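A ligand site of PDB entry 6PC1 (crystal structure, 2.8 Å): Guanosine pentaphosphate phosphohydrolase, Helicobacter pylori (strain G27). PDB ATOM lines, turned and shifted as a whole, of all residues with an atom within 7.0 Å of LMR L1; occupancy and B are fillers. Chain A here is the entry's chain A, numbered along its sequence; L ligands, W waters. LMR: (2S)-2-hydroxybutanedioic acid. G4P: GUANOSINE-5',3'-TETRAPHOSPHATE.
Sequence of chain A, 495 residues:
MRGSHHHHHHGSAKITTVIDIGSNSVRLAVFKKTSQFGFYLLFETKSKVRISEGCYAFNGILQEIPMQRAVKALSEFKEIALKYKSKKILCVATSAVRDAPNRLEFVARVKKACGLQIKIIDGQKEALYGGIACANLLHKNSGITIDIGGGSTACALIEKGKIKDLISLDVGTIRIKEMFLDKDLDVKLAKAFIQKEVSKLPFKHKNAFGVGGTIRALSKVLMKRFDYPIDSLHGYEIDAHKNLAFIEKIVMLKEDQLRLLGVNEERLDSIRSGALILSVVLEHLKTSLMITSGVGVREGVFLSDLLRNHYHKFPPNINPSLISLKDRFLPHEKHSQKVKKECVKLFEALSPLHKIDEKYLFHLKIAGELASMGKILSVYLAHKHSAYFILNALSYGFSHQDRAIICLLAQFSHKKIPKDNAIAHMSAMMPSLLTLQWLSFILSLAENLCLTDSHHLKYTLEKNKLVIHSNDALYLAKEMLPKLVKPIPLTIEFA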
ATOM      1  N   ASP A  20       4.797 -22.348  15.901  1.00  0.00           N
ATOM      2  CA  ASP A  20       4.798 -21.040  16.563  1.00  0.00           C
ATOM      3  C   ASP A  20       4.610 -21.271  18.058  1.00  0.00           C
ATOM      4  O   ASP A  20       3.506 -21.636  18.495  1.00  0.00           O
ATOM      5  CB  ASP A  20       3.704 -20.143  15.985  1.00  0.00           C
ATOM      6  CG  ASP A  20       3.745 -18.731  16.546  1.00  0.00           C
ATOM      7  OD1 ASP A  20       4.393 -18.516  17.594  1.00  0.00           O
ATOM      8  OD2 ASP A  20       3.112 -17.849  15.936  1.00  0.00           O
ATOM      9  N   GLY A  22       3.829 -19.761  21.012  1.00  0.00           N
ATOM     10  CA  GLY A  22       3.260 -18.529  21.505  1.00  0.00           C
ATOM     11  C   GLY A  22       3.187 -18.480  23.025  1.00  0.00           C
ATOM     12  O   GLY A  22       3.492 -19.439  23.720  1.00  0.00           O
ATOM     13  N   SER A  23       2.763 -17.319  23.522  1.00  0.00           N
ATOM     14  CA  SER A  23       2.652 -17.126  24.964  1.00  0.00           C
ATOM     15  C   SER A  23       1.429 -17.841  25.527  1.00  0.00           C
ATOM     16  O   SER A  23       1.495 -18.428  26.609  1.00  0.00           O
ATOM     17  CB  SER A  23       2.573 -15.629  25.286  1.00  0.00           C
ATOM     18  OG  SER A  23       3.608 -14.919  24.618  1.00  0.00           O
ATOM     19  N   ASN A  24       0.314 -17.818  24.793  1.00  0.00           N
ATOM     20  CA  ASN A  24      -0.923 -18.439  25.223  1.00  0.00           C
ATOM     21  C   ASN A  24      -1.119 -19.834  24.649  1.00  0.00           C
ATOM     22  O   ASN A  24      -1.690 -20.693  25.335  1.00  0.00           O
ATOM     23  CB  ASN A  24      -2.120 -17.562  24.829  1.00  0.00           C
ATOM     24  CG  ASN A  24      -3.414 -18.012  25.457  1.00  0.00           C
ATOM     25  OD1 ASN A  24      -3.425 -18.535  26.577  1.00  0.00           O
ATOM     26  ND2 ASN A  24      -4.522 -17.820  24.747  1.00  0.00           N
ATOM     27  N   SER A  25      -0.659 -20.080  23.427  1.00  0.00           N
ATOM     28  CA  SER A  25      -0.872 -21.361  22.769  1.00  0.00           C
ATOM     29  C   SER A  25       0.338 -21.709  21.926  1.00  0.00           C
ATOM     30  O   SER A  25       1.128 -20.842  21.548  1.00  0.00           O
ATOM     31  CB  SER A  25      -2.122 -21.349  21.881  1.00  0.00           C
ATOM     32  OG  SER A  25      -1.968 -20.439  20.799  1.00  0.00           O
ATOM     33  N   VAL A  26       0.475 -23.001  21.633  1.00  0.00           N
ATOM     34  CA  VAL A  26       1.511 -23.506  20.737  1.00  0.00           C
ATOM     35  C   VAL A  26       0.817 -23.968  19.460  1.00  0.00           C
ATOM     36  O   VAL A  26      -0.106 -24.791  19.507  1.00  0.00           O
ATOM     37  CB  VAL A  26       2.302 -24.656  21.384  1.00  0.00           C
ATOM     38  CG1 VAL A  26       3.479 -25.043  20.513  1.00  0.00           C
ATOM     39  CG2 VAL A  26       2.781 -24.249  22.766  1.00  0.00           C
ATOM     40  N   ARG A  27       1.251 -23.428  18.327  1.00  0.00           N
ATOM     41  CA  ARG A  27       0.567 -23.612  17.049  1.00  0.00           C
ATOM     42  C   ARG A  27       1.439 -24.392  16.072  1.00  0.00           C
ATOM     43  O   ARG A  27       2.666 -24.259  16.051  1.00  0.00           O
ATOM     44  CB  ARG A  27       0.199 -22.251  16.440  1.00  0.00           C
ATOM     45  CG  ARG A  27      -0.701 -21.401  17.323  1.00  0.00           C
ATOM     46  CD  ARG A  27      -2.162 -21.717  17.087  1.00  0.00           C
ATOM     47  NE  ARG A  27      -3.046 -20.976  17.981  1.00  0.00           N
ATOM     48  CZ  ARG A  27      -4.370 -21.001  17.919  1.00  0.00           C
ATOM     49  NH1 ARG A  27      -4.981 -21.731  16.990  1.00  0.00           N
ATOM     50  NH2 ARG A  27      -5.096 -20.297  18.779  1.00  0.00           N
ATOM     51  N   ASP A 147      -1.491  -7.185  15.971  1.00  0.00           N
ATOM     52  CA  ASP A 147      -1.287  -8.573  16.362  1.00  0.00           C
ATOM     53  C   ASP A 147      -1.265  -8.640  17.883  1.00  0.00           C
ATOM     54  O   ASP A 147      -0.213  -8.506  18.509  1.00  0.00           O
ATOM     55  CB  ASP A 147      -0.012  -9.144  15.756  1.00  0.00           C
ATOM     56  CG  ASP A 147       0.181 -10.614  16.053  1.00  0.00           C
ATOM     57  OD1 ASP A 147      -0.561 -11.166  16.892  1.00  0.00           O
ATOM     58  OD2 ASP A 147       1.086 -11.229  15.458  1.00  0.00           O
ATOM     59  N   ILE A 148      -2.432  -8.854  18.472  1.00  0.00           N
ATOM     60  CA  ILE A 148      -2.571  -8.936  19.927  1.00  0.00           C
ATOM     61  C   ILE A 148      -2.393 -10.397  20.327  1.00  0.00           C
ATOM     62  O   ILE A 148      -3.220 -11.250  20.004  1.00  0.00           O
ATOM     63  CB  ILE A 148      -3.925  -8.398  20.407  1.00  0.00           C
ATOM     64  CG1 ILE A 148      -4.046  -6.913  20.054  1.00  0.00           C
ATOM     65  CG2 ILE A 148      -4.073  -8.594  21.909  1.00  0.00           C
ATOM     66  CD1 ILE A 148      -5.449  -6.351  20.226  1.00  0.00           C
ATOM     67  N   GLY A 149      -1.302 -10.682  21.039  1.00  0.00           N
ATOM     68  CA  GLY A 149      -1.030 -11.997  21.560  1.00  0.00           C
ATOM     69  C   GLY A 149      -1.111 -12.043  23.071  1.00  0.00           C
ATOM     70  O   GLY A 149      -1.702 -11.167  23.728  1.00  0.00           O
ATOM     71  N   GLY A 150      -0.509 -13.089  23.639  1.00  0.00           N
ATOM     72  CA  GLY A 150      -0.594 -13.293  25.082  1.00  0.00           C
ATOM     73  C   GLY A 150       0.304 -12.384  25.889  1.00  0.00           C
ATOM     74  O   GLY A 150      -0.016 -12.080  27.048  1.00  0.00           O
ATOM     75  N   THR A 173      -2.832 -10.188  26.322  1.00  0.00           N
ATOM     76  CA  THR A 173      -4.026 -10.683  26.997  1.00  0.00           C
ATOM     77  C   THR A 173      -3.672 -11.270  28.369  1.00  0.00           C
ATOM     78  O   THR A 173      -4.101 -10.755  29.403  1.00  0.00           O
ATOM     79  CB  THR A 173      -4.715 -11.734  26.129  1.00  0.00           C
ATOM     80  OG1 THR A 173      -3.806 -12.804  25.852  1.00  0.00           O
ATOM     81  CG2 THR A 173      -5.201 -11.122  24.823  1.00  0.00           C
ATOM     82  N   ILE A 174      -2.882 -12.342  28.367  1.00  0.00           N
ATOM     83  CA  ILE A 174      -2.533 -13.015  29.624  1.00  0.00           C
ATOM     84  C   ILE A 174      -1.809 -12.060  30.560  1.00  0.00           C
ATOM     85  O   ILE A 174      -1.940 -12.178  31.794  1.00  0.00           O
ATOM     86  CB  ILE A 174      -1.690 -14.269  29.324  1.00  0.00           C
ATOM     87  CG1 ILE A 174      -2.400 -15.160  28.300  1.00  0.00           C
ATOM     88  CG2 ILE A 174      -1.414 -15.055  30.606  1.00  0.00           C
ATOM     89  CD1 ILE A 174      -3.814 -15.579  28.679  1.00  0.00           C
ATOM     90  N   VAL A 211      -4.936  -9.134  13.610  1.00  0.00           N
ATOM     91  CA  VAL A 211      -4.235 -10.413  13.574  1.00  0.00           C
ATOM     92  C   VAL A 211      -4.282 -11.024  14.967  1.00  0.00           C
ATOM     93  O   VAL A 211      -4.266 -10.319  15.978  1.00  0.00           O
ATOM     94  CB  VAL A 211      -2.774 -10.257  13.101  1.00  0.00           C
ATOM     95  CG1 VAL A 211      -2.042 -11.595  13.115  1.00  0.00           C
ATOM     96  CG2 VAL A 211      -2.726  -9.634  11.715  1.00  0.00           C
ATOM     97  N   GLY A 212      -4.345 -12.340  15.019  1.00  0.00           N
ATOM     98  CA  GLY A 212      -4.288 -13.066  16.268  1.00  0.00           C
ATOM     99  C   GLY A 212      -5.634 -13.641  16.661  1.00  0.00           C
ATOM    100  O   GLY A 212      -6.697 -13.236  16.167  1.00  0.00           O
ATOM    101  N   GLY A 213      -5.587 -14.611  17.583  1.00  0.00           N
ATOM    102  CA  GLY A 213      -6.787 -15.322  17.965  1.00  0.00           C
ATOM    103  C   GLY A 213      -7.772 -14.477  18.758  1.00  0.00           C
ATOM    104  O   GLY A 213      -8.977 -14.708  18.693  1.00  0.00           O
ATOM    105  N   THR A 214      -7.281 -13.486  19.502  1.00  0.00           N
ATOM    106  CA  THR A 214      -8.177 -12.589  20.219  1.00  0.00           C
ATOM    107  C   THR A 214      -9.093 -11.866  19.240  1.00  0.00           C
ATOM    108  O   THR A 214     -10.315 -11.858  19.394  1.00  0.00           O
ATOM    109  CB  THR A 214      -7.380 -11.589  21.052  1.00  0.00           C
ATOM    110  OG1 THR A 214      -6.779 -12.254  22.167  1.00  0.00           O
ATOM    111  CG2 THR A 214      -8.267 -10.448  21.559  1.00  0.00           C
ATOM    112  N   ARG A 216      -9.657 -12.610  16.094  1.00  0.00           N
ATOM    113  CA  ARG A 216     -10.495 -13.582  15.406  1.00  0.00           C
ATOM    114  C   ARG A 216     -11.696 -13.958  16.262  1.00  0.00           C
ATOM    115  O   ARG A 216     -12.810 -14.144  15.750  1.00  0.00           O
ATOM    116  CB  ARG A 216      -9.692 -14.830  15.049  1.00  0.00           C
ATOM    117  CG  ARG A 216      -8.606 -14.607  13.994  1.00  0.00           C
ATOM    118  CD  ARG A 216      -8.121 -15.918  13.397  1.00  0.00           C
ATOM    119  NE  ARG A 216      -7.905 -16.937  14.419  1.00  0.00           N
ATOM    120  CZ  ARG A 216      -6.742 -17.213  15.005  1.00  0.00           C
ATOM    121  NH1 ARG A 216      -5.644 -16.539  14.676  1.00  0.00           N
ATOM    122  NH2 ARG A 216      -6.676 -18.161  15.929  1.00  0.00           N
ATOM    123  N   ARG A 267     -11.253 -19.165  25.478  1.00  0.00           N
ATOM    124  CA  ARG A 267     -11.037 -17.741  25.256  1.00  0.00           C
ATOM    125  C   ARG A 267     -11.720 -16.861  26.308  1.00  0.00           C
ATOM    126  O   ARG A 267     -11.526 -15.642  26.290  1.00  0.00           O
ATOM    127  CB  ARG A 267     -11.548 -17.321  23.872  1.00  0.00           C
ATOM    128  CG  ARG A 267     -10.695 -17.804  22.708  1.00  0.00           C
ATOM    129  CD  ARG A 267      -9.448 -16.953  22.536  1.00  0.00           C
ATOM    130  NE  ARG A 267      -8.561 -17.495  21.514  1.00  0.00           N
ATOM    131  CZ  ARG A 267      -7.314 -17.073  21.303  1.00  0.00           C
ATOM    132  NH1 ARG A 267      -6.802 -16.101  22.049  1.00  0.00           N
ATOM    133  NH2 ARG A 267      -6.588 -17.633  20.350  1.00  0.00           N
ATOM    134  N   SER A 270      -9.316 -14.742  28.461  1.00  0.00           N
ATOM    135  CA  SER A 270      -8.411 -13.827  27.787  1.00  0.00           C
ATOM    136  C   SER A 270      -9.080 -12.835  26.837  1.00  0.00           C
ATOM    137  O   SER A 270      -8.421 -11.871  26.426  1.00  0.00           O
ATOM    138  CB  SER A 270      -7.358 -14.626  26.995  1.00  0.00           C
ATOM    139  OG  SER A 270      -7.957 -15.475  26.038  1.00  0.00           O
ATOM    140  N   GLY A 296      -1.130 -14.738   9.955  1.00  0.00           N
ATOM    141  CA  GLY A 296      -0.301 -14.025  10.919  1.00  0.00           C
ATOM    142  C   GLY A 296       1.140 -14.432  10.842  1.00  0.00           C
ATOM    143  O   GLY A 296       1.681 -14.665   9.750  1.00  0.00           O
ATOM    144  N   VAL A 297       1.788 -14.519  12.009  1.00  0.00           N
ATOM    145  CA  VAL A 297       3.215 -14.805  12.073  1.00  0.00           C
ATOM    146  C   VAL A 297       3.546 -16.096  11.328  1.00  0.00           C
ATOM    147  O   VAL A 297       4.516 -16.157  10.571  1.00  0.00           O
ATOM    148  CB  VAL A 297       3.685 -14.862  13.538  1.00  0.00           C
ATOM    149  CG1 VAL A 297       5.162 -15.240  13.636  1.00  0.00           C
ATOM    150  CG2 VAL A 297       3.435 -13.525  14.230  1.00  0.00           C
ATOM    151  N   ARG A 298       2.739 -17.141  11.551  1.00  0.00           N
ATOM    152  CA  ARG A 298       3.028 -18.428  10.936  1.00  0.00           C
ATOM    153  C   ARG A 298       3.126 -18.311   9.417  1.00  0.00           C
ATOM    154  O   ARG A 298       4.053 -18.827   8.797  1.00  0.00           O
ATOM    155  CB  ARG A 298       1.965 -19.453  11.336  1.00  0.00           C
ATOM    156  CG  ARG A 298       2.101 -19.940  12.769  1.00  0.00           C
ATOM    157  CD  ARG A 298       0.972 -20.880  13.160  1.00  0.00           C
ATOM    158  NE  ARG A 298      -0.321 -20.201  13.217  1.00  0.00           N
ATOM    159  CZ  ARG A 298      -0.673 -19.348  14.176  1.00  0.00           C
ATOM    160  NH1 ARG A 298       0.165 -19.060  15.160  1.00  0.00           N
ATOM    161  NH2 ARG A 298      -1.874 -18.784  14.142  1.00  0.00           N
HETATM  162  C1  LMR L   1      -2.331 -16.986  17.234  1.00  0.00           C
HETATM  163  O1A LMR L   1      -3.410 -17.218  16.738  1.00  0.00           O
HETATM  164  O1B LMR L   1      -1.214 -17.093  16.497  1.00  0.00           O
HETATM  165  C2  LMR L   1      -2.236 -16.582  18.682  1.00  0.00           C
HETATM  166  O2  LMR L   1      -2.385 -15.165  18.794  1.00  0.00           O
HETATM  167  C3  LMR L   1      -3.321 -17.277  19.489  1.00  0.00           C
HETATM  168  C4  LMR L   1      -3.402 -16.627  20.847  1.00  0.00           C
HETATM  169  O4A LMR L   1      -3.444 -15.423  20.938  1.00  0.00           O
HETATM  170  O4B LMR L   1      -3.437 -17.381  21.949  1.00  0.00           O
HETATM  171  PB  G4P L   2     -14.940 -26.012  13.085  1.00  0.00           P
HETATM  172  O1B G4P L   2     -15.951 -25.211  13.820  1.00  0.00           O
HETATM  173  O2B G4P L   2     -15.691 -27.240  12.369  1.00  0.00           O
HETATM  174  O3B G4P L   2     -13.849 -26.599  14.113  1.00  0.00           O
HETATM  175  O3A G4P L   2     -14.206 -25.135  11.948  1.00  0.00           O
HETATM  176  PA  G4P L   2     -14.050 -23.599  12.424  1.00  0.00           P
HETATM  177  O1A G4P L   2     -13.418 -22.824  11.323  1.00  0.00           O
HETATM  178  O2A G4P L   2     -15.493 -22.956  12.748  1.00  0.00           O
HETATM  179  O5' G4P L   2     -13.114 -23.503  13.736  1.00  0.00           O
HETATM  180  C5' G4P L   2     -11.837 -24.066  13.407  1.00  0.00           C
HETATM  181  C4' G4P L   2     -10.719 -23.199  13.985  1.00  0.00           C
HETATM  182  O4' G4P L   2     -10.101 -22.428  12.919  1.00  0.00           O
HETATM  183  C3' G4P L   2     -11.230 -22.149  15.006  1.00  0.00           C
HETATM  184  O3' G4P L   2     -10.181 -21.841  15.924  1.00  0.00           O
HETATM  185  C2' G4P L   2     -11.486 -20.934  14.102  1.00  0.00           C
HETATM  186  O2' G4P L   2     -11.556 -19.732  14.870  1.00  0.00           O
HETATM  187  C1' G4P L   2     -10.203 -21.030  13.266  1.00  0.00           C
HETATM  188  N9  G4P L   2     -10.219 -20.225  12.035  1.00  0.00           N
HETATM  189  C8  G4P L   2     -11.258 -20.007  11.185  1.00  0.00           C
HETATM  190  N7  G4P L   2     -10.861 -19.265  10.199  1.00  0.00           N
HETATM  191  C5  G4P L   2      -9.552 -18.965  10.357  1.00  0.00           C
HETATM  192  C6  G4P L   2      -8.611 -18.204   9.619  1.00  0.00           C
HETATM  193  O6  G4P L   2      -8.923 -17.646   8.579  1.00  0.00           O
HETATM  194  N1  G4P L   2      -7.347 -18.128  10.092  1.00  0.00           N
HETATM  195  C2  G4P L   2      -6.995 -18.751  11.244  1.00  0.00           C
HETATM  196  N2  G4P L   2      -5.703 -18.655  11.708  1.00  0.00           N
HETATM  197  N3  G4P L   2      -7.864 -19.455  11.939  1.00  0.00           N
HETATM  198  C4  G4P L   2      -9.125 -19.577  11.538  1.00  0.00           C
HETATM  199  PC  G4P L   2     -10.669 -22.143  17.426  1.00  0.00           P
HETATM  200  O1C G4P L   2     -10.999 -23.583  17.554  1.00  0.00           O
HETATM  201  O2C G4P L   2     -11.976 -21.272  17.764  1.00  0.00           O
HETATM  202  O3C G4P L   2      -9.484 -21.772  18.445  1.00  0.00           O
HETATM  203  PD  G4P L   2      -8.617 -20.541  17.872  1.00  0.00           P
HETATM  204  O1D G4P L   2      -9.448 -19.663  17.022  1.00  0.00           O
HETATM  205  O2D G4P L   2      -8.044 -19.697  19.113  1.00  0.00           O
HETATM  206  O3D G4P L   2      -7.371 -21.097  17.009  1.00  0.00           O
HETATM  207  O   HOH W   1       0.856 -15.978  19.395  1.00  0.00           O
HETATM  208  O   HOH W   2      -4.620 -12.992  21.005  1.00  0.00           O
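Residues that only touch LMR L1: Ser 25 (3.6 Å) and Gly 212 (3.8 Å). Within 4 Å of LMR L1: Asn 24, Ser 25, Arg 27, Gly 212, Gly 213, Arg 216, Arg 267 and Arg 298.
The guanidinium group of Arg 267 is in salt-bridge range of an oxygen (O4B) of LMR L1, at 3.5 Å. The guanidinium group (NH1) of Arg 216 is in salt-bridge range of an oxygen (O1A) of LMR L1 (3.1 Å). An oxygen (O2) of LMR L1 sits at hydrogen-bond distance from the backbone NH of Gly 213. O4B of LMR L1 lies within hydrogen-bond range of ND2 of Asn 24. The guanidinium group (NH2) of Arg 216 lies within salt-bridge range of an oxygen (O3D) of G4P L2. The guanidinium group (NH1) of Arg 298 is in salt-bridge range of an oxygen (O1B) of LMR L1 (2.7 Å). An oxygen (O1A) of LMR L1 is in salt-bridge range of the guanidinium group of Arg 27 (3.97 Å). NH2 of Arg 267 is in salt-bridge range of O2D of G4P L2. The guanidinium group (NH1) of Arg 27 lies within salt-bridge range of an oxygen (O3D) of G4P L2, 2.5 Å away.
The guanidinium group of Arg 27 lies within hydrogen-bond range of the side-chain hydroxyl of Ser 25, 3.1 Å away. The backbone carbonyl oxygen (O) of Arg 27 lies within hydrogen-bond range of the backbone NH (N) of Asp 20. NH1 of Arg 298 is in salt-bridge range of OD2 of Asp 20, 3.3 Å away.
Water W2 lies within hydrogen-bond range of the backbone carbonyl oxygen of Ile 148 (2.4 Å), the side-chain hydroxyl of Thr 214 (2.6 Å) and an oxygen (O4A) of LMR L1 (2.7 Å).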
